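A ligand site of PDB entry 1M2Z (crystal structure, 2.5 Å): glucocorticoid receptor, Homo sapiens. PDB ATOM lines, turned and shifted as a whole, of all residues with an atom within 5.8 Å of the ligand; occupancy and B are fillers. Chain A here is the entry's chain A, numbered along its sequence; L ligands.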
ATOM      1  N   MET A  40       4.266  23.317  -8.299  1.00  0.00           N
ATOM      2  CA  MET A  40       3.427  23.870  -9.360  1.00  0.00           C
ATOM      3  C   MET A  40       3.388  25.391  -9.335  1.00  0.00           C
ATOM      4  O   MET A  40       3.529  26.034 -10.365  1.00  0.00           O
ATOM      5  CB  MET A  40       2.028  23.329  -9.229  1.00  0.00           C
ATOM      6  CG  MET A  40       1.977  21.833  -8.999  1.00  0.00           C
ATOM      7  SD  MET A  40       1.046  20.967 -10.244  1.00  0.00           S
ATOM      8  CE  MET A  40      -0.611  21.184  -9.634  1.00  0.00           C
ATOM      9  N   LEU A  43       6.440  26.764 -10.601  1.00  0.00           N
ATOM     10  CA  LEU A  43       6.495  26.554 -12.042  1.00  0.00           C
ATOM     11  C   LEU A  43       5.602  27.537 -12.793  1.00  0.00           C
ATOM     12  O   LEU A  43       5.918  27.932 -13.904  1.00  0.00           O
ATOM     13  CB  LEU A  43       6.109  25.097 -12.393  1.00  0.00           C
ATOM     14  CG  LEU A  43       7.057  23.988 -11.879  1.00  0.00           C
ATOM     15  CD1 LEU A  43       6.603  22.648 -12.415  1.00  0.00           C
ATOM     16  CD2 LEU A  43       8.491  24.285 -12.310  1.00  0.00           C
ATOM     17  N   ASN A  44       4.487  27.921 -12.189  1.00  0.00           N
ATOM     18  CA  ASN A  44       3.581  28.877 -12.832  1.00  0.00           C
ATOM     19  C   ASN A  44       4.240  30.249 -12.894  1.00  0.00           C
ATOM     20  O   ASN A  44       4.182  30.914 -13.926  1.00  0.00           O
ATOM     21  CB  ASN A  44       2.250  28.977 -12.062  1.00  0.00           C
ATOM     22  CG  ASN A  44       1.350  27.790 -12.294  1.00  0.00           C
ATOM     23  OD1 ASN A  44       1.163  27.343 -13.420  1.00  0.00           O
ATOM     24  ND2 ASN A  44       0.762  27.269 -11.221  1.00  0.00           N
ATOM     25  N   LEU A  46       7.366  30.824 -12.877  1.00  0.00           N
ATOM     26  CA  LEU A  46       8.423  30.660 -13.875  1.00  0.00           C
ATOM     27  C   LEU A  46       7.800  30.784 -15.255  1.00  0.00           C
ATOM     28  O   LEU A  46       8.369  31.416 -16.149  1.00  0.00           O
ATOM     29  CB  LEU A  46       9.088  29.280 -13.720  1.00  0.00           C
ATOM     30  CG  LEU A  46      10.157  28.925 -14.768  1.00  0.00           C
ATOM     31  CD1 LEU A  46      11.296  29.922 -14.692  1.00  0.00           C
ATOM     32  CD2 LEU A  46      10.662  27.511 -14.523  1.00  0.00           C
ATOM     33  N   GLY A  47       6.641  30.166 -15.441  1.00  0.00           N
ATOM     34  CA  GLY A  47       5.949  30.218 -16.716  1.00  0.00           C
ATOM     35  C   GLY A  47       5.604  31.652 -17.090  1.00  0.00           C
ATOM     36  O   GLY A  47       5.689  32.012 -18.266  1.00  0.00           O
ATOM     37  N   GLN A  50       8.675  33.232 -18.385  1.00  0.00           N
ATOM     38  CA  GLN A  50       9.063  32.596 -19.646  1.00  0.00           C
ATOM     39  C   GLN A  50       8.171  33.069 -20.781  1.00  0.00           C
ATOM     40  O   GLN A  50       8.626  33.231 -21.915  1.00  0.00           O
ATOM     41  CB  GLN A  50       8.967  31.092 -19.540  1.00  0.00           C
ATOM     42  CG  GLN A  50      10.181  30.423 -18.897  1.00  0.00           C
ATOM     43  CD  GLN A  50      10.093  28.906 -18.980  1.00  0.00           C
ATOM     44  OE1 GLN A  50      11.020  28.198 -18.576  1.00  0.00           O
ATOM     45  NE2 GLN A  50       8.985  28.399 -19.512  1.00  0.00           N
ATOM     46  N   TRP A  80       1.185  29.597 -26.333  1.00  0.00           N
ATOM     47  CA  TRP A  80       2.133  29.863 -25.260  1.00  0.00           C
ATOM     48  C   TRP A  80       2.489  28.551 -24.564  1.00  0.00           C
ATOM     49  O   TRP A  80       3.620  28.360 -24.114  1.00  0.00           O
ATOM     50  CB  TRP A  80       1.536  30.856 -24.210  1.00  0.00           C
ATOM     51  CG  TRP A  80       0.449  30.278 -23.359  1.00  0.00           C
ATOM     52  CD1 TRP A  80      -0.861  30.112 -23.702  1.00  0.00           C
ATOM     53  CD2 TRP A  80       0.593  29.732 -22.040  1.00  0.00           C
ATOM     54  NE1 TRP A  80      -1.538  29.491 -22.675  1.00  0.00           N
ATOM     55  CE2 TRP A  80      -0.674  29.254 -21.640  1.00  0.00           C
ATOM     56  CE3 TRP A  80       1.678  29.608 -21.152  1.00  0.00           C
ATOM     57  CZ2 TRP A  80      -0.890  28.655 -20.394  1.00  0.00           C
ATOM     58  CZ3 TRP A  80       1.463  29.010 -19.916  1.00  0.00           C
ATOM     59  CH2 TRP A  80       0.192  28.541 -19.556  1.00  0.00           C
ATOM     60  N   MET A  81       1.524  27.637 -24.488  1.00  0.00           N
ATOM     61  CA  MET A  81       1.713  26.341 -23.862  1.00  0.00           C
ATOM     62  C   MET A  81       2.601  25.466 -24.733  1.00  0.00           C
ATOM     63  O   MET A  81       3.502  24.792 -24.249  1.00  0.00           O
ATOM     64  CB  MET A  81       0.367  25.660 -23.628  1.00  0.00           C
ATOM     65  CG  MET A  81       0.452  24.330 -22.878  1.00  0.00           C
ATOM     66  SD  MET A  81       1.251  24.514 -21.274  1.00  0.00           S
ATOM     67  CE  MET A  81      -0.109  25.114 -20.284  1.00  0.00           C
ATOM     68  N   MET A  84       6.245  26.838 -24.550  1.00  0.00           N
ATOM     69  CA  MET A  84       6.832  26.528 -23.252  1.00  0.00           C
ATOM     70  C   MET A  84       7.070  25.038 -23.045  1.00  0.00           C
ATOM     71  O   MET A  84       8.112  24.634 -22.521  1.00  0.00           O
ATOM     72  CB  MET A  84       5.937  27.093 -22.133  1.00  0.00           C
ATOM     73  CG  MET A  84       6.335  28.492 -21.630  1.00  0.00           C
ATOM     74  SD  MET A  84       6.920  29.631 -22.911  1.00  0.00           S
ATOM     75  CE  MET A  84       8.694  29.606 -22.590  1.00  0.00           C
ATOM     76  N   ALA A  85       6.106  24.214 -23.450  1.00  0.00           N
ATOM     77  CA  ALA A  85       6.219  22.765 -23.300  1.00  0.00           C
ATOM     78  C   ALA A  85       7.312  22.218 -24.227  1.00  0.00           C
ATOM     79  O   ALA A  85       8.051  21.318 -23.845  1.00  0.00           O
ATOM     80  CB  ALA A  85       4.887  22.099 -23.606  1.00  0.00           C
ATOM     81  N   LEU A  88      10.605  23.175 -22.925  1.00  0.00           N
ATOM     82  CA  LEU A  88      10.837  22.338 -21.763  1.00  0.00           C
ATOM     83  C   LEU A  88      11.419  21.007 -22.204  1.00  0.00           C
ATOM     84  O   LEU A  88      12.474  20.587 -21.730  1.00  0.00           O
ATOM     85  CB  LEU A  88       9.528  22.090 -21.024  1.00  0.00           C
ATOM     86  CG  LEU A  88       9.576  21.111 -19.843  1.00  0.00           C
ATOM     87  CD1 LEU A  88      10.544  21.621 -18.789  1.00  0.00           C
ATOM     88  CD2 LEU A  88       8.186  20.938 -19.259  1.00  0.00           C
ATOM     89  N   ARG A  91      15.111  21.326 -23.196  1.00  0.00           N
ATOM     90  CA  ARG A  91      16.062  21.386 -22.095  1.00  0.00           C
ATOM     91  C   ARG A  91      16.176  20.049 -21.363  1.00  0.00           C
ATOM     92  O   ARG A  91      17.233  19.700 -20.858  1.00  0.00           O
ATOM     93  CB  ARG A  91      15.654  22.478 -21.092  1.00  0.00           C
ATOM     94  CG  ARG A  91      15.694  23.911 -21.664  1.00  0.00           C
ATOM     95  CD  ARG A  91      15.553  24.954 -20.545  1.00  0.00           C
ATOM     96  NE  ARG A  91      14.355  24.727 -19.749  1.00  0.00           N
ATOM     97  CZ  ARG A  91      13.119  25.032 -20.135  1.00  0.00           C
ATOM     98  NH1 ARG A  91      12.889  25.591 -21.318  1.00  0.00           N
ATOM     99  NH2 ARG A  91      12.091  24.754 -19.338  1.00  0.00           N
ATOM    100  N   PHE A 103      12.675  21.896 -15.970  1.00  0.00           N
ATOM    101  CA  PHE A 103      11.990  23.171 -16.106  1.00  0.00           C
ATOM    102  C   PHE A 103      12.998  24.312 -16.038  1.00  0.00           C
ATOM    103  O   PHE A 103      12.825  25.363 -16.664  1.00  0.00           O
ATOM    104  CB  PHE A 103      10.935  23.339 -15.009  1.00  0.00           C
ATOM    105  CG  PHE A 103       9.745  22.437 -15.167  1.00  0.00           C
ATOM    106  CD1 PHE A 103       9.781  21.126 -14.731  1.00  0.00           C
ATOM    107  CD2 PHE A 103       8.597  22.914 -15.797  1.00  0.00           C
ATOM    108  CE1 PHE A 103       8.688  20.279 -14.913  1.00  0.00           C
ATOM    109  CE2 PHE A 103       7.498  22.076 -15.980  1.00  0.00           C
ATOM    110  CZ  PHE A 103       7.548  20.761 -15.542  1.00  0.00           C
ATOM    111  N   MET A 119       1.756  15.031  -9.659  1.00  0.00           N
ATOM    112  CA  MET A 119       2.879  15.410 -10.519  1.00  0.00           C
ATOM    113  C   MET A 119       3.048  14.575 -11.795  1.00  0.00           C
ATOM    114  O   MET A 119       3.194  15.137 -12.886  1.00  0.00           O
ATOM    115  CB  MET A 119       4.184  15.378  -9.727  1.00  0.00           C
ATOM    116  CG  MET A 119       5.292  16.302 -10.295  1.00  0.00           C
ATOM    117  SD  MET A 119       5.211  18.004  -9.660  1.00  0.00           S
ATOM    118  CE  MET A 119       4.297  18.830 -10.965  1.00  0.00           C
ATOM    119  N   GLN A 122       0.594  15.000 -14.761  1.00  0.00           N
ATOM    120  CA  GLN A 122       0.852  16.255 -15.460  1.00  0.00           C
ATOM    121  C   GLN A 122       2.121  16.128 -16.294  1.00  0.00           C
ATOM    122  O   GLN A 122       2.079  16.216 -17.518  1.00  0.00           O
ATOM    123  CB  GLN A 122       1.017  17.382 -14.452  1.00  0.00           C
ATOM    124  CG  GLN A 122      -0.175  17.590 -13.573  1.00  0.00           C
ATOM    125  CD  GLN A 122       0.050  18.650 -12.522  1.00  0.00           C
ATOM    126  OE1 GLN A 122       0.358  19.796 -12.827  1.00  0.00           O
ATOM    127  NE2 GLN A 122      -0.119  18.265 -11.262  1.00  0.00           N
ATOM    128  N   CYS A 123       3.230  15.909 -15.605  1.00  0.00           N
ATOM    129  CA  CYS A 123       4.541  15.767 -16.235  1.00  0.00           C
ATOM    130  C   CYS A 123       4.579  14.721 -17.341  1.00  0.00           C
ATOM    131  O   CYS A 123       5.370  14.844 -18.283  1.00  0.00           O
ATOM    132  CB  CYS A 123       5.585  15.416 -15.161  1.00  0.00           C
ATOM    133  SG  CYS A 123       5.760  16.629 -13.841  1.00  0.00           S
ATOM    134  N   MET A 126       4.573  16.109 -20.720  1.00  0.00           N
ATOM    135  CA  MET A 126       5.757  16.926 -20.953  1.00  0.00           C
ATOM    136  C   MET A 126       6.925  16.012 -21.316  1.00  0.00           C
ATOM    137  O   MET A 126       7.647  16.255 -22.282  1.00  0.00           O
ATOM    138  CB  MET A 126       6.077  17.745 -19.717  1.00  0.00           C
ATOM    139  CG  MET A 126       5.093  18.892 -19.472  1.00  0.00           C
ATOM    140  SD  MET A 126       5.258  19.655 -17.854  1.00  0.00           S
ATOM    141  CE  MET A 126       3.674  19.244 -17.123  1.00  0.00           C
ATOM    142  N   ASN A 211      -3.901  18.310 -23.610  1.00  0.00           N
ATOM    143  CA  ASN A 211      -3.853  17.671 -22.307  1.00  0.00           C
ATOM    144  C   ASN A 211      -3.251  18.581 -21.233  1.00  0.00           C
ATOM    145  O   ASN A 211      -3.808  18.717 -20.155  1.00  0.00           O
ATOM    146  CB  ASN A 211      -3.039  16.360 -22.384  1.00  0.00           C
ATOM    147  CG  ASN A 211      -3.861  15.210 -22.922  1.00  0.00           C
ATOM    148  OD1 ASN A 211      -4.890  14.842 -22.356  1.00  0.00           O
ATOM    149  ND2 ASN A 211      -3.410  14.628 -24.029  1.00  0.00           N
ATOM    150  N   LEU A 212      -2.125  19.211 -21.551  1.00  0.00           N
ATOM    151  CA  LEU A 212      -1.478  20.120 -20.605  1.00  0.00           C
ATOM    152  C   LEU A 212      -2.401  21.293 -20.285  1.00  0.00           C
ATOM    153  O   LEU A 212      -2.451  21.764 -19.154  1.00  0.00           O
ATOM    154  CB  LEU A 212      -0.154  20.660 -21.191  1.00  0.00           C
ATOM    155  CG  LEU A 212       1.007  19.678 -21.374  1.00  0.00           C
ATOM    156  CD1 LEU A 212       2.202  20.420 -21.968  1.00  0.00           C
ATOM    157  CD2 LEU A 212       1.372  19.052 -20.042  1.00  0.00           C
ATOM    158  N   LEU A 213      -3.129  21.750 -21.300  1.00  0.00           N
ATOM    159  CA  LEU A 213      -4.046  22.874 -21.161  1.00  0.00           C
ATOM    160  C   LEU A 213      -5.277  22.524 -20.337  1.00  0.00           C
ATOM    161  O   LEU A 213      -5.699  23.324 -19.498  1.00  0.00           O
ATOM    162  CB  LEU A 213      -4.452  23.381 -22.546  1.00  0.00           C
ATOM    163  CG  LEU A 213      -4.441  24.902 -22.748  1.00  0.00           C
ATOM    164  CD1 LEU A 213      -3.146  25.484 -22.204  1.00  0.00           C
ATOM    165  CD2 LEU A 213      -4.605  25.223 -24.219  1.00  0.00           C
ATOM    166  N   TYR A 215      -5.403  20.443 -18.091  1.00  0.00           N
ATOM    167  CA  TYR A 215      -4.866  20.349 -16.746  1.00  0.00           C
ATOM    168  C   TYR A 215      -4.468  21.725 -16.223  1.00  0.00           C
ATOM    169  O   TYR A 215      -4.310  21.914 -15.010  1.00  0.00           O
ATOM    170  CB  TYR A 215      -3.657  19.424 -16.736  1.00  0.00           C
ATOM    171  CG  TYR A 215      -3.498  18.676 -15.437  1.00  0.00           C
ATOM    172  CD1 TYR A 215      -3.315  19.356 -14.230  1.00  0.00           C
ATOM    173  CD2 TYR A 215      -3.561  17.282 -15.398  1.00  0.00           C
ATOM    174  CE1 TYR A 215      -3.213  18.676 -13.025  1.00  0.00           C
ATOM    175  CE2 TYR A 215      -3.463  16.588 -14.193  1.00  0.00           C
ATOM    176  CZ  TYR A 215      -3.279  17.290 -13.016  1.00  0.00           C
ATOM    177  OH  TYR A 215      -3.177  16.611 -11.821  1.00  0.00           O
ATOM    178  N   CYS A 216      -4.303  22.688 -17.120  1.00  0.00           N
ATOM    179  CA  CYS A 216      -3.937  24.053 -16.729  1.00  0.00           C
ATOM    180  C   CYS A 216      -5.176  24.846 -16.311  1.00  0.00           C
ATOM    181  O   CYS A 216      -5.132  25.632 -15.373  1.00  0.00           O
ATOM    182  CB  CYS A 216      -3.248  24.769 -17.905  1.00  0.00           C
ATOM    183  SG  CYS A 216      -2.859  26.517 -17.582  1.00  0.00           S
ATOM    184  N   PHE A 217      -6.280  24.627 -17.022  1.00  0.00           N
ATOM    185  CA  PHE A 217      -7.532  25.315 -16.716  1.00  0.00           C
ATOM    186  C   PHE A 217      -8.173  24.746 -15.466  1.00  0.00           C
ATOM    187  O   PHE A 217      -8.606  25.481 -14.587  1.00  0.00           O
ATOM    188  CB  PHE A 217      -8.524  25.194 -17.900  1.00  0.00           C
ATOM    189  CG  PHE A 217      -7.998  25.729 -19.207  1.00  0.00           C
ATOM    190  CD1 PHE A 217      -7.190  26.865 -19.231  1.00  0.00           C
ATOM    191  CD2 PHE A 217      -8.344  25.128 -20.414  1.00  0.00           C
ATOM    192  CE1 PHE A 217      -6.733  27.386 -20.443  1.00  0.00           C
ATOM    193  CE2 PHE A 217      -7.895  25.644 -21.626  1.00  0.00           C
ATOM    194  CZ  PHE A 217      -7.083  26.771 -21.640  1.00  0.00           C
ATOM    195  N   THR A 219      -6.865  23.435 -12.947  1.00  0.00           N
ATOM    196  CA  THR A 219      -6.142  23.852 -11.757  1.00  0.00           C
ATOM    197  C   THR A 219      -6.396  25.336 -11.485  1.00  0.00           C
ATOM    198  O   THR A 219      -6.638  25.739 -10.356  1.00  0.00           O
ATOM    199  CB  THR A 219      -4.622  23.639 -11.915  1.00  0.00           C
ATOM    200  OG1 THR A 219      -4.389  22.440 -12.668  1.00  0.00           O
ATOM    201  CG2 THR A 219      -3.969  23.485 -10.552  1.00  0.00           C
ATOM    202  N   ILE A 227      -3.322  27.005  -5.955  1.00  0.00           N
ATOM    203  CA  ILE A 227      -2.134  26.958  -6.794  1.00  0.00           C
ATOM    204  C   ILE A 227      -2.142  28.226  -7.639  1.00  0.00           C
ATOM    205  O   ILE A 227      -2.879  28.342  -8.616  1.00  0.00           O
ATOM    206  CB  ILE A 227      -2.140  25.707  -7.692  1.00  0.00           C
ATOM    207  CG1 ILE A 227      -1.861  24.471  -6.830  1.00  0.00           C
ATOM    208  CG2 ILE A 227      -1.123  25.841  -8.811  1.00  0.00           C
ATOM    209  CD1 ILE A 227      -1.995  23.162  -7.556  1.00  0.00           C
ATOM    210  N   PHE A 229      -1.134  31.458 -10.085  1.00  0.00           N
ATOM    211  CA  PHE A 229      -0.689  31.701 -11.449  1.00  0.00           C
ATOM    212  C   PHE A 229      -0.286  33.168 -11.457  1.00  0.00           C
ATOM    213  O   PHE A 229      -0.971  34.003 -10.844  1.00  0.00           O
ATOM    214  CB  PHE A 229      -1.841  31.479 -12.454  1.00  0.00           C
ATOM    215  CG  PHE A 229      -2.108  30.035 -12.768  1.00  0.00           C
ATOM    216  CD1 PHE A 229      -2.598  29.162 -11.801  1.00  0.00           C
ATOM    217  CD2 PHE A 229      -1.895  29.540 -14.060  1.00  0.00           C
ATOM    218  CE1 PHE A 229      -2.860  27.826 -12.095  1.00  0.00           C
ATOM    219  CE2 PHE A 229      -2.148  28.209 -14.363  1.00  0.00           C
ATOM    220  CZ  PHE A 229      -2.635  27.350 -13.386  1.00  0.00           C
ATOM    221  N   LEU A 233       0.247  34.738 -16.926  1.00  0.00           N
ATOM    222  CA  LEU A 233      -0.498  33.512 -17.229  1.00  0.00           C
ATOM    223  C   LEU A 233      -1.995  33.650 -16.921  1.00  0.00           C
ATOM    224  O   LEU A 233      -2.820  33.244 -17.725  1.00  0.00           O
ATOM    225  CB  LEU A 233       0.088  32.315 -16.448  1.00  0.00           C
ATOM    226  CG  LEU A 233       1.142  31.460 -17.198  1.00  0.00           C
ATOM    227  CD1 LEU A 233       2.264  32.336 -17.715  1.00  0.00           C
ATOM    228  CD2 LEU A 233       1.678  30.389 -16.258  1.00  0.00           C
HETATM  229  C1  LIG L   1       6.155  26.323 -16.713  1.00  0.00           C
HETATM  230  C2  LIG L   1       7.470  26.244 -16.892  1.00  0.00           C
HETATM  231  C3  LIG L   1       7.963  25.566 -18.137  1.00  0.00           C
HETATM  232  C4  LIG L   1       6.954  24.932 -19.045  1.00  0.00           C
HETATM  233  C5  LIG L   1       5.659  25.049 -18.794  1.00  0.00           C
HETATM  234  C6  LIG L   1       4.714  24.370 -19.738  1.00  0.00           C
HETATM  235  C7  LIG L   1       3.761  23.475 -18.960  1.00  0.00           C
HETATM  236  C8  LIG L   1       3.148  24.162 -17.742  1.00  0.00           C
HETATM  237  C9  LIG L   1       4.152  24.885 -16.854  1.00  0.00           C
HETATM  238  C10 LIG L   1       5.084  25.815 -17.623  1.00  0.00           C
HETATM  239  C11 LIG L   1       3.579  25.436 -15.545  1.00  0.00           C
HETATM  240  C12 LIG L   1       2.544  24.571 -14.852  1.00  0.00           C
HETATM  241  C13 LIG L   1       1.488  24.023 -15.822  1.00  0.00           C
HETATM  242  C14 LIG L   1       2.203  23.271 -16.934  1.00  0.00           C
HETATM  243  C15 LIG L   1       1.131  22.422 -17.615  1.00  0.00           C
HETATM  244  C16 LIG L   1       0.163  22.086 -16.485  1.00  0.00           C
HETATM  245  C17 LIG L   1       0.639  22.879 -15.269  1.00  0.00           C
HETATM  246  C18 LIG L   1       0.591  25.163 -16.302  1.00  0.00           C
HETATM  247  C19 LIG L   1       4.400  27.055 -18.181  1.00  0.00           C
HETATM  248  C20 LIG L   1      -0.494  23.320 -14.365  1.00  0.00           C
HETATM  249  C21 LIG L   1      -0.444  23.188 -12.860  1.00  0.00           C
HETATM  250  C22 LIG L   1       0.054  20.576 -16.299  1.00  0.00           C
HETATM  251  F1  LIG L   1       4.956  23.887 -16.389  1.00  0.00           F
HETATM  252  O1  LIG L   1       9.161  25.555 -18.404  1.00  0.00           O
HETATM  253  O2  LIG L   1       2.947  26.693 -15.798  1.00  0.00           O
HETATM  254  O3  LIG L   1       1.456  22.003 -14.502  1.00  0.00           O
HETATM  255  O4  LIG L   1      -1.505  23.825 -14.846  1.00  0.00           O
HETATM  256  O5  LIG L   1      -0.691  24.444 -12.248  1.00  0.00           O
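The side-chain hydroxyl (OG1) of Thr 219 lies within hydrogen-bond range of the backbone carbonyl oxygen (O) of Tyr 215 (2.4 Å). The side-chain amide nitrogen (ND2) of Asn 44 is in hydrogen-bond range of the backbone carbonyl oxygen (O) of Met 40. The side-chain amide oxygen of Gln 122 sits close to the side-chain sulfur of Met 40 (2.9 Å). The backbone carbonyl oxygen (O) of Phe 103 is in hydrogen-bond range of the guanidinium group (NH2) of Arg 91, at 2.8 Å.
An oxygen (O1) of the ligand is in hydrogen-bond range of the side-chain amide nitrogen of Gln 50 (3.1 Å). O1 of the ligand lies within hydrogen-bond range of NH2 of Arg 91 (3.2 Å). OE1 of Gln 122 is in hydrogen-bond range of O3 of the ligand. OD1 of Asn 44 sits at hydrogen-bond distance from O2 of the ligand.
O of Tyr 215 sits close to O4 of the ligand (3.4 Å). Merely in contact with the ligand: Met 40 (3.7 Å), Leu 43 (3.2 Å), Gly 47 (3.8 Å), Trp 80 (3.9 Å), Met 81 (3.6 Å), Met 84 (3.7 Å), Ala 85 (3.97 Å), Phe 103 (3.1 Å), Met 126 (3.9 Å), Leu 212 (3.7 Å), Cys 216 (3.1 Å), Thr 219 (3.8 Å), Ile 227 (3.7 Å), Phe 229 (3.7 Å) and Leu 233 (3.9 Å). Hydrophobic or aromatic side chains within 4 Å of the ligand: Met 40, Trp 80, Met 81, Met 84, Phe 103, Met 126, Tyr 215, Ile 227, Phe 229 and Leu 233. Within 4 Å of the ligand: Met 40, Leu 43, Asn 44, Gly 47, Gln 50, Trp 80, Met 81, Met 84, Ala 85, Arg 91, Phe 103, Gln 122, Met 126, Leu 212, Tyr 215, Cys 216, Thr 219, Ile 227, Phe 229 and Leu 233.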
